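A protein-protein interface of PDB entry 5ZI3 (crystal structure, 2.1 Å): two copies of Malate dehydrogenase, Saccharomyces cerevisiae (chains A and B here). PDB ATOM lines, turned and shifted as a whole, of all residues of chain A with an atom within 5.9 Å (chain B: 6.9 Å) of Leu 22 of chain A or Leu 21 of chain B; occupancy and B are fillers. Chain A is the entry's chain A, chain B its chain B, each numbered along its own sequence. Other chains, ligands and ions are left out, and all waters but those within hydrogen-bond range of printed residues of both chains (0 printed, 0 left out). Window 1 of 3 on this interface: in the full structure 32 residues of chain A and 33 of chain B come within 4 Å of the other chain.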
ATOM      1  N   GLN A  17     -14.516  -9.337 -25.021  1.00  0.00           N
ATOM      2  CA  GLN A  17     -13.943 -10.187 -26.082  1.00  0.00           C
ATOM      3  C   GLN A  17     -14.634 -11.547 -26.138  1.00  0.00           C
ATOM      4  O   GLN A  17     -15.105 -11.907 -27.149  1.00  0.00           O
ATOM      5  CB  GLN A  17     -12.466 -10.402 -25.901  1.00  0.00           C
ATOM      6  CG  GLN A  17     -11.672  -9.195 -26.197  1.00  0.00           C
ATOM      7  CD  GLN A  17     -10.263  -9.565 -26.558  1.00  0.00           C
ATOM      8  OE1 GLN A  17     -10.007 -10.582 -27.193  1.00  0.00           O
ATOM      9  NE2 GLN A  17      -9.344  -8.752 -26.111  1.00  0.00           N
ATOM     10  N   PRO A  18     -14.670 -12.302 -25.028  1.00  0.00           N
ATOM     11  CA  PRO A  18     -15.460 -13.541 -25.078  1.00  0.00           C
ATOM     12  C   PRO A  18     -16.960 -13.309 -25.393  1.00  0.00           C
ATOM     13  O   PRO A  18     -17.577 -14.097 -26.110  1.00  0.00           O
ATOM     14  CB  PRO A  18     -15.218 -14.178 -23.699  1.00  0.00           C
ATOM     15  CG  PRO A  18     -14.639 -13.109 -22.853  1.00  0.00           C
ATOM     16  CD  PRO A  18     -13.960 -12.130 -23.753  1.00  0.00           C
ATOM     17  N   LEU A  19     -17.527 -12.186 -24.956  1.00  0.00           N
ATOM     18  CA  LEU A  19     -18.926 -11.929 -25.291  1.00  0.00           C
ATOM     19  C   LEU A  19     -19.076 -11.728 -26.794  1.00  0.00           C
ATOM     20  O   LEU A  19     -20.073 -12.138 -27.398  1.00  0.00           O
ATOM     21  CB  LEU A  19     -19.439 -10.706 -24.553  1.00  0.00           C
ATOM     22  CG  LEU A  19     -20.826 -10.200 -24.862  1.00  0.00           C
ATOM     23  CD1 LEU A  19     -21.818 -11.230 -24.322  1.00  0.00           C
ATOM     24  CD2 LEU A  19     -21.039  -8.837 -24.163  1.00  0.00           C
ATOM     25  N   SER A  20     -18.115 -11.043 -27.395  1.00  0.00           N
ATOM     26  CA  SER A  20     -18.141 -10.784 -28.834  1.00  0.00           C
ATOM     27  C   SER A  20     -18.040 -12.123 -29.653  1.00  0.00           C
ATOM     28  O   SER A  20     -18.750 -12.329 -30.622  1.00  0.00           O
ATOM     29  CB  SER A  20     -17.016  -9.791 -29.205  1.00  0.00           C
ATOM     30  OG  SER A  20     -17.216  -8.527 -28.582  1.00  0.00           O
ATOM     31  N   LEU A  21     -17.157 -13.021 -29.242  1.00  0.00           N
ATOM     32  CA  LEU A  21     -17.039 -14.343 -29.874  1.00  0.00           C
ATOM     33  C   LEU A  21     -18.397 -15.111 -29.836  1.00  0.00           C
ATOM     34  O   LEU A  21     -18.937 -15.506 -30.864  1.00  0.00           O
ATOM     35  CB  LEU A  21     -15.912 -15.102 -29.180  1.00  0.00           C
ATOM     36  CG  LEU A  21     -15.875 -16.606 -29.549  1.00  0.00           C
ATOM     37  CD1 LEU A  21     -15.642 -16.809 -31.049  1.00  0.00           C
ATOM     38  CD2 LEU A  21     -14.902 -17.380 -28.666  1.00  0.00           C
ATOM     39  N   LEU A  22     -19.001 -15.210 -28.643  1.00  0.00           N
ATOM     40  CA  LEU A  22     -20.285 -15.918 -28.489  1.00  0.00           C
ATOM     41  C   LEU A  22     -21.341 -15.265 -29.328  1.00  0.00           C
ATOM     42  O   LEU A  22     -22.028 -15.935 -30.056  1.00  0.00           O
ATOM     43  CB  LEU A  22     -20.689 -15.986 -27.027  1.00  0.00           C
ATOM     44  CG  LEU A  22     -19.686 -16.853 -26.276  1.00  0.00           C
ATOM     45  CD1 LEU A  22     -19.940 -16.779 -24.797  1.00  0.00           C
ATOM     46  CD2 LEU A  22     -19.675 -18.309 -26.761  1.00  0.00           C
ATOM     47  N   LEU A  23     -21.408 -13.940 -29.301  1.00  0.00           N
ATOM     48  CA  LEU A  23     -22.317 -13.225 -30.155  1.00  0.00           C
ATOM     49  C   LEU A  23     -22.059 -13.469 -31.657  1.00  0.00           C
ATOM     50  O   LEU A  23     -23.006 -13.585 -32.370  1.00  0.00           O
ATOM     51  CB  LEU A  23     -22.381 -11.736 -29.836  1.00  0.00           C
ATOM     52  CG  LEU A  23     -23.572 -11.290 -28.935  1.00  0.00           C
ATOM     53  CD1 LEU A  23     -24.869 -11.270 -29.691  1.00  0.00           C
ATOM     54  CD2 LEU A  23     -23.754 -12.188 -27.769  1.00  0.00           C
ATOM     55  N   LYS A  24     -20.808 -13.577 -32.115  1.00  0.00           N
ATOM     56  CA  LYS A  24     -20.562 -13.974 -33.513  1.00  0.00           C
ATOM     57  C   LYS A  24     -21.199 -15.312 -33.898  1.00  0.00           C
ATOM     58  O   LYS A  24     -21.607 -15.487 -35.042  1.00  0.00           O
ATOM     59  CB  LYS A  24     -19.078 -14.060 -33.824  1.00  0.00           C
ATOM     60  CG  LYS A  24     -18.751 -14.414 -35.281  1.00  0.00           C
ATOM     61  CD  LYS A  24     -19.170 -13.289 -36.204  1.00  0.00           C
ATOM     62  CE  LYS A  24     -18.704 -13.550 -37.632  1.00  0.00           C
ATOM     63  NZ  LYS A  24     -19.752 -14.151 -38.472  1.00  0.00           N
ATOM     64  N   LEU A  25     -21.264 -16.249 -32.964  1.00  0.00           N
ATOM     65  CA  LEU A  25     -21.876 -17.516 -33.225  1.00  0.00           C
ATOM     66  C   LEU A  25     -23.412 -17.522 -33.324  1.00  0.00           C
ATOM     67  O   LEU A  25     -23.993 -18.538 -33.682  1.00  0.00           O
ATOM     68  CB  LEU A  25     -21.470 -18.503 -32.158  1.00  0.00           C
ATOM     69  CG  LEU A  25     -19.975 -18.622 -31.962  1.00  0.00           C
ATOM     70  CD1 LEU A  25     -19.712 -19.793 -31.085  1.00  0.00           C
ATOM     71  CD2 LEU A  25     -19.304 -18.781 -33.310  1.00  0.00           C
ATOM     72  N   SER A  26     -24.092 -16.443 -32.947  1.00  0.00           N
ATOM     73  CA  SER A  26     -25.552 -16.503 -32.864  1.00  0.00           C
ATOM     74  C   SER A  26     -26.215 -16.467 -34.243  1.00  0.00           C
ATOM     75  O   SER A  26     -25.988 -15.553 -35.004  1.00  0.00           O
ATOM     76  CB  SER A  26     -26.127 -15.346 -32.027  1.00  0.00           C
ATOM     77  OG  SER A  26     -27.540 -15.205 -32.256  1.00  0.00           O
ATOM     78  N   LEU A 237     -15.256 -14.939 -18.057  1.00  0.00           N
ATOM     79  CA  LEU A 237     -15.709 -15.938 -19.007  1.00  0.00           C
ATOM     80  C   LEU A 237     -17.235 -16.376 -18.772  1.00  0.00           C
ATOM     81  O   LEU A 237     -18.039 -16.362 -19.694  1.00  0.00           O
ATOM     82  CB  LEU A 237     -14.698 -17.090 -19.018  1.00  0.00           C
ATOM     83  CG  LEU A 237     -13.273 -16.813 -19.497  1.00  0.00           C
ATOM     84  CD1 LEU A 237     -12.401 -18.057 -19.327  1.00  0.00           C
ATOM     85  CD2 LEU A 237     -13.245 -16.401 -20.951  1.00  0.00           C
ATOM     86  N   SER A 238     -17.628 -16.635 -17.536  1.00  0.00           N
ATOM     87  CA  SER A 238     -19.035 -16.933 -17.224  1.00  0.00           C
ATOM     88  C   SER A 238     -19.955 -15.725 -17.341  1.00  0.00           C
ATOM     89  O   SER A 238     -21.082 -15.881 -17.767  1.00  0.00           O
ATOM     90  CB  SER A 238     -19.189 -17.614 -15.835  1.00  0.00           C
ATOM     91  OG  SER A 238     -18.361 -17.099 -14.843  1.00  0.00           O
ATOM     92  N   ALA A 240     -19.507 -13.452 -19.584  1.00  0.00           N
ATOM     93  CA  ALA A 240     -19.742 -13.425 -21.027  1.00  0.00           C
ATOM     94  C   ALA A 240     -20.763 -14.481 -21.547  1.00  0.00           C
ATOM     95  O   ALA A 240     -21.599 -14.196 -22.403  1.00  0.00           O
ATOM     96  CB  ALA A 240     -18.387 -13.636 -21.738  1.00  0.00           C
ATOM     97  N   PHE A 241     -20.636 -15.711 -21.048  1.00  0.00           N
ATOM     98  CA  PHE A 241     -21.587 -16.764 -21.308  1.00  0.00           C
ATOM     99  C   PHE A 241     -23.001 -16.349 -20.929  1.00  0.00           C
ATOM    100  O   PHE A 241     -23.941 -16.424 -21.778  1.00  0.00           O
ATOM    101  CB  PHE A 241     -21.221 -18.024 -20.512  1.00  0.00           C
ATOM    102  CG  PHE A 241     -22.235 -19.099 -20.609  1.00  0.00           C
ATOM    103  CD1 PHE A 241     -22.374 -19.841 -21.793  1.00  0.00           C
ATOM    104  CD2 PHE A 241     -23.070 -19.378 -19.550  1.00  0.00           C
ATOM    105  CE1 PHE A 241     -23.286 -20.854 -21.898  1.00  0.00           C
ATOM    106  CE2 PHE A 241     -24.012 -20.406 -19.644  1.00  0.00           C
ATOM    107  CZ  PHE A 241     -24.136 -21.125 -20.831  1.00  0.00           C
ATOM    108  N   ALA A 244     -24.243 -13.553 -23.302  1.00  0.00           N
ATOM    109  CA  ALA A 244     -24.652 -14.029 -24.652  1.00  0.00           C
ATOM    110  C   ALA A 244     -25.960 -14.803 -24.556  1.00  0.00           C
ATOM    111  O   ALA A 244     -26.781 -14.702 -25.419  1.00  0.00           O
ATOM    112  CB  ALA A 244     -23.594 -14.937 -25.261  1.00  0.00           C
ATOM    113  N   ILE B   8      -6.529 -29.266 -21.354  1.00  0.00           N
ATOM    114  CA  ILE B   8      -5.987 -28.138 -22.124  1.00  0.00           C
ATOM    115  C   ILE B   8      -4.681 -27.639 -21.529  1.00  0.00           C
ATOM    116  O   ILE B   8      -4.578 -27.166 -20.370  1.00  0.00           O
ATOM    117  CB  ILE B   8      -6.988 -26.990 -22.286  1.00  0.00           C
ATOM    118  CG1 ILE B   8      -8.285 -27.555 -22.868  1.00  0.00           C
ATOM    119  CG2 ILE B   8      -6.385 -25.854 -23.164  1.00  0.00           C
ATOM    120  CD1 ILE B   8      -9.369 -26.528 -22.984  1.00  0.00           C
ATOM    121  N   GLY B  16      -5.871 -20.044 -25.502  1.00  0.00           N
ATOM    122  CA  GLY B  16      -6.251 -20.974 -24.513  1.00  0.00           C
ATOM    123  C   GLY B  16      -7.489 -20.657 -23.744  1.00  0.00           C
ATOM    124  O   GLY B  16      -8.262 -21.575 -23.410  1.00  0.00           O
ATOM    125  N   GLN B  17      -7.722 -19.375 -23.486  1.00  0.00           N
ATOM    126  CA  GLN B  17      -8.848 -18.979 -22.612  1.00  0.00           C
ATOM    127  C   GLN B  17     -10.189 -19.105 -23.255  1.00  0.00           C
ATOM    128  O   GLN B  17     -11.065 -19.725 -22.654  1.00  0.00           O
ATOM    129  CB  GLN B  17      -8.694 -17.549 -22.092  1.00  0.00           C
ATOM    130  CG  GLN B  17      -7.714 -17.440 -20.977  1.00  0.00           C
ATOM    131  CD  GLN B  17      -7.948 -16.175 -20.141  1.00  0.00           C
ATOM    132  OE1 GLN B  17      -9.061 -15.694 -20.007  1.00  0.00           O
ATOM    133  NE2 GLN B  17      -6.883 -15.634 -19.611  1.00  0.00           N
ATOM    134  N   PRO B  18     -10.375 -18.512 -24.459  1.00  0.00           N
ATOM    135  CA  PRO B  18     -11.613 -18.757 -25.241  1.00  0.00           C
ATOM    136  C   PRO B  18     -11.814 -20.209 -25.681  1.00  0.00           C
ATOM    137  O   PRO B  18     -12.959 -20.659 -25.763  1.00  0.00           O
ATOM    138  CB  PRO B  18     -11.462 -17.835 -26.487  1.00  0.00           C
ATOM    139  CG  PRO B  18     -10.006 -17.427 -26.496  1.00  0.00           C
ATOM    140  CD  PRO B  18      -9.563 -17.440 -25.079  1.00  0.00           C
ATOM    141  N   LEU B  19     -10.726 -20.928 -25.951  1.00  0.00           N
ATOM    142  CA  LEU B  19     -10.842 -22.385 -26.211  1.00  0.00           C
ATOM    143  C   LEU B  19     -11.442 -23.142 -24.981  1.00  0.00           C
ATOM    144  O   LEU B  19     -12.281 -24.013 -25.114  1.00  0.00           O
ATOM    145  CB  LEU B  19      -9.495 -22.972 -26.525  1.00  0.00           C
ATOM    146  CG  LEU B  19      -9.429 -24.423 -27.036  1.00  0.00           C
ATOM    147  CD1 LEU B  19     -10.203 -24.651 -28.330  1.00  0.00           C
ATOM    148  CD2 LEU B  19      -7.940 -24.748 -27.171  1.00  0.00           C
ATOM    149  N   SER B  20     -10.990 -22.792 -23.792  1.00  0.00           N
ATOM    150  CA  SER B  20     -11.455 -23.438 -22.580  1.00  0.00           C
ATOM    151  C   SER B  20     -12.938 -23.158 -22.386  1.00  0.00           C
ATOM    152  O   SER B  20     -13.734 -24.085 -22.051  1.00  0.00           O
ATOM    153  CB  SER B  20     -10.624 -22.996 -21.371  1.00  0.00           C
ATOM    154  OG  SER B  20      -9.237 -23.282 -21.591  1.00  0.00           O
ATOM    155  N   LEU B  21     -13.344 -21.919 -22.671  1.00  0.00           N
ATOM    156  CA  LEU B  21     -14.780 -21.545 -22.640  1.00  0.00           C
ATOM    157  C   LEU B  21     -15.594 -22.368 -23.633  1.00  0.00           C
ATOM    158  O   LEU B  21     -16.696 -22.848 -23.314  1.00  0.00           O
ATOM    159  CB  LEU B  21     -14.992 -20.026 -22.923  1.00  0.00           C
ATOM    160  CG  LEU B  21     -16.423 -19.564 -23.162  1.00  0.00           C
ATOM    161  CD1 LEU B  21     -17.301 -19.903 -21.973  1.00  0.00           C
ATOM    162  CD2 LEU B  21     -16.516 -18.053 -23.460  1.00  0.00           C
ATOM    163  N   LEU B  22     -15.096 -22.492 -24.863  1.00  0.00           N
ATOM    164  CA  LEU B  22     -15.876 -23.191 -25.865  1.00  0.00           C
ATOM    165  C   LEU B  22     -16.017 -24.690 -25.464  1.00  0.00           C
ATOM    166  O   LEU B  22     -17.105 -25.299 -25.582  1.00  0.00           O
ATOM    167  CB  LEU B  22     -15.293 -22.975 -27.279  1.00  0.00           C
ATOM    168  CG  LEU B  22     -15.368 -21.528 -27.784  1.00  0.00           C
ATOM    169  CD1 LEU B  22     -14.951 -21.419 -29.249  1.00  0.00           C
ATOM    170  CD2 LEU B  22     -16.746 -20.901 -27.650  1.00  0.00           C
ATOM    171  N   LEU B  23     -14.945 -25.244 -24.948  1.00  0.00           N
ATOM    172  CA  LEU B  23     -14.950 -26.654 -24.525  1.00  0.00           C
ATOM    173  C   LEU B  23     -15.900 -26.965 -23.365  1.00  0.00           C
ATOM    174  O   LEU B  23     -16.543 -28.029 -23.413  1.00  0.00           O
ATOM    175  CB  LEU B  23     -13.567 -27.132 -24.159  1.00  0.00           C
ATOM    176  CG  LEU B  23     -12.844 -27.877 -25.307  1.00  0.00           C
ATOM    177  CD1 LEU B  23     -13.483 -29.230 -25.595  1.00  0.00           C
ATOM    178  CD2 LEU B  23     -12.741 -27.068 -26.575  1.00  0.00           C
ATOM    179  N   LYS B  24     -15.967 -26.043 -22.369  1.00  0.00           N
ATOM    180  CA  LYS B  24     -16.894 -26.118 -21.245  1.00  0.00           C
ATOM    181  C   LYS B  24     -18.332 -26.199 -21.747  1.00  0.00           C
ATOM    182  O   LYS B  24     -19.159 -26.796 -21.103  1.00  0.00           O
ATOM    183  CB  LYS B  24     -16.734 -24.938 -20.259  1.00  0.00           C
ATOM    184  CG  LYS B  24     -17.738 -24.938 -19.103  1.00  0.00           C
ATOM    185  CD  LYS B  24     -17.359 -26.049 -18.109  1.00  0.00           C
ATOM    186  CE  LYS B  24     -18.313 -26.195 -16.936  1.00  0.00           C
ATOM    187  NZ  LYS B  24     -19.469 -26.993 -17.345  1.00  0.00           N
ATOM    188  N   LEU B  25     -18.603 -25.635 -22.903  1.00  0.00           N
ATOM    189  CA  LEU B  25     -19.926 -25.711 -23.524  1.00  0.00           C
ATOM    190  C   LEU B  25     -20.263 -27.019 -24.261  1.00  0.00           C
ATOM    191  O   LEU B  25     -21.440 -27.231 -24.620  1.00  0.00           O
ATOM    192  CB  LEU B  25     -20.152 -24.574 -24.513  1.00  0.00           C
ATOM    193  CG  LEU B  25     -19.851 -23.143 -24.048  1.00  0.00           C
ATOM    194  CD1 LEU B  25     -20.406 -22.179 -25.064  1.00  0.00           C
ATOM    195  CD2 LEU B  25     -20.388 -22.837 -22.664  1.00  0.00           C
ATOM    196  N   SER B  26     -19.276 -27.878 -24.466  1.00  0.00           N
ATOM    197  CA  SER B  26     -19.473 -29.112 -25.227  1.00  0.00           C
ATOM    198  C   SER B  26     -20.262 -30.103 -24.424  1.00  0.00           C
ATOM    199  O   SER B  26     -19.806 -30.512 -23.381  1.00  0.00           O
ATOM    200  CB  SER B  26     -18.147 -29.802 -25.538  1.00  0.00           C
ATOM    201  OG  SER B  26     -18.403 -30.998 -26.246  1.00  0.00           O
ATOM    202  N   LEU B  32     -13.113 -31.544 -17.708  1.00  0.00           N
ATOM    203  CA  LEU B  32     -12.290 -30.592 -18.401  1.00  0.00           C
ATOM    204  C   LEU B  32     -11.239 -30.157 -17.411  1.00  0.00           C
ATOM    205  O   LEU B  32     -11.588 -29.653 -16.357  1.00  0.00           O
ATOM    206  CB  LEU B  32     -13.134 -29.415 -18.923  1.00  0.00           C
ATOM    207  CG  LEU B  32     -12.466 -28.280 -19.702  1.00  0.00           C
ATOM    208  CD1 LEU B  32     -11.794 -28.812 -20.938  1.00  0.00           C
ATOM    209  CD2 LEU B  32     -13.482 -27.238 -20.147  1.00  0.00           C
ATOM    210  N   LEU B  34      -7.820 -27.859 -16.988  1.00  0.00           N
ATOM    211  CA  LEU B  34      -7.065 -26.744 -17.502  1.00  0.00           C
ATOM    212  C   LEU B  34      -5.671 -26.607 -16.871  1.00  0.00           C
ATOM    213  O   LEU B  34      -5.529 -26.628 -15.639  1.00  0.00           O
ATOM    214  CB  LEU B  34      -7.878 -25.461 -17.369  1.00  0.00           C
ATOM    215  CG  LEU B  34      -9.308 -25.584 -17.871  1.00  0.00           C
ATOM    216  CD1 LEU B  34      -9.950 -24.221 -17.703  1.00  0.00           C
ATOM    217  CD2 LEU B  34      -9.331 -26.006 -19.330  1.00  0.00           C
ATOM    218  N   ILE B  43      -9.167 -19.537 -13.868  1.00  0.00           N
ATOM    219  CA  ILE B  43      -9.988 -19.646 -15.041  1.00  0.00           C
ATOM    220  C   ILE B  43     -10.885 -20.884 -14.936  1.00  0.00           C
ATOM    221  O   ILE B  43     -12.055 -20.845 -15.280  1.00  0.00           O
ATOM    222  CB  ILE B  43      -9.097 -19.760 -16.312  1.00  0.00           C
ATOM    223  CG1 ILE B  43      -8.558 -18.363 -16.666  1.00  0.00           C
ATOM    224  CG2 ILE B  43      -9.907 -20.261 -17.492  1.00  0.00           C
ATOM    225  CD1 ILE B  43      -7.242 -18.363 -17.406  1.00  0.00           C
ATOM    226  N   LEU B  47     -14.962 -20.836 -15.105  1.00  0.00           N
ATOM    227  CA  LEU B  47     -15.725 -21.747 -16.000  1.00  0.00           C
ATOM    228  C   LEU B  47     -16.572 -22.823 -15.242  1.00  0.00           C
ATOM    229  O   LEU B  47     -17.605 -23.229 -15.750  1.00  0.00           O
ATOM    230  CB  LEU B  47     -14.790 -22.497 -16.991  1.00  0.00           C
ATOM    231  CG  LEU B  47     -14.128 -21.580 -18.000  1.00  0.00           C
ATOM    232  CD1 LEU B  47     -13.066 -22.237 -18.893  1.00  0.00           C
ATOM    233  CD2 LEU B  47     -15.190 -20.919 -18.848  1.00  0.00           C
ATOM    234  N   ILE B  50     -20.514 -22.254 -15.141  1.00  0.00           N
ATOM    235  CA  ILE B  50     -21.392 -22.396 -16.306  1.00  0.00           C
ATOM    236  C   ILE B  50     -22.279 -23.630 -16.188  1.00  0.00           C
ATOM    237  O   ILE B  50     -21.828 -24.663 -15.804  1.00  0.00           O
ATOM    238  CB  ILE B  50     -20.588 -22.382 -17.619  1.00  0.00           C
ATOM    239  CG1 ILE B  50     -20.042 -20.962 -17.806  1.00  0.00           C
ATOM    240  CG2 ILE B  50     -21.432 -22.662 -18.852  1.00  0.00           C
ATOM    241  CD1 ILE B  50     -19.075 -20.800 -18.960  1.00  0.00           C
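Of the 15 printed residues of chain A, 4 touch a printed residue of chain B. Hydrophobic or aromatic side chains of chain A within 4 Å of the printed part of chain B: Leu 22, Leu 237 and Phe 241. Along chain A the printed residues that touch a printed residue of chain B span positions 22 to 241. Printed residues of chain B that touch a printed residue of chain A: Gln 17, Leu 21, Leu 25, Ile 43, Leu 47 and Ile 50. Along chain B the printed residues that touch a printed residue of chain A span positions 17 to 50. Among the printed residues, no Asp or Glu carboxylate lies within 4 Å of a Lys or Arg side-chain nitrogen of the other chain.
CD1 of Leu 22 of chain A touches CD2 of Leu 21 of chain B (3.9 Å). Gln 17 of chain B touches Leu 237 of chain A (O to CD1, 3.95 Å). Ile 43 of chain B touches Leu 237 of chain A. Leu 237 of chain A touches Leu 47 of chain B (CB to CD2, 3.9 Å). Ser 238 of chain A touches Ile 50 of chain B (CB to CG1, 3.98 Å). CE1 of Phe 241 of chain A touches CD2 of Leu 25 of chain B, at 3.6 Å. Ile 50 of chain B touches Phe 241 of chain A (CG2 to CE2, 3.5 Å).
Leu 22 of chain A touches Leu 21 of chain B, but with the chains exchanged Leu 21 of chain A does not touch Leu 22 of chain B (4.1 Å). Positions printed for both chains: 17, 18, 19, 20, 21, 22, 23, 24, 25 and 26. Of the 7 pairs that touch across the chains among the printed residues, none has its exchanged pair printed and touching as well.
Of the printed residues of chain B, Leu 22 of chain A touches Leu 21 (3.9 Å). Of the printed residues of chain B, Ser 238 of chain A touches Ile 50. Of the printed residues of chain A, Gln 17 of chain B touches Leu 237. Leu 21 of chain B touches just one residue of chain A: Leu 22 (3.9 Å). Leu 34 of chain B touches none of the printed residues of chain A. Of the printed residues of chain A, Ile 50 of chain B touches Ser 238 (3.98 Å) and Phe 241 (3.5 Å). The nearest printed residue of chain B that does not touch Leu 22 of chain A is Leu 22 of chain B (4.01 Å).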
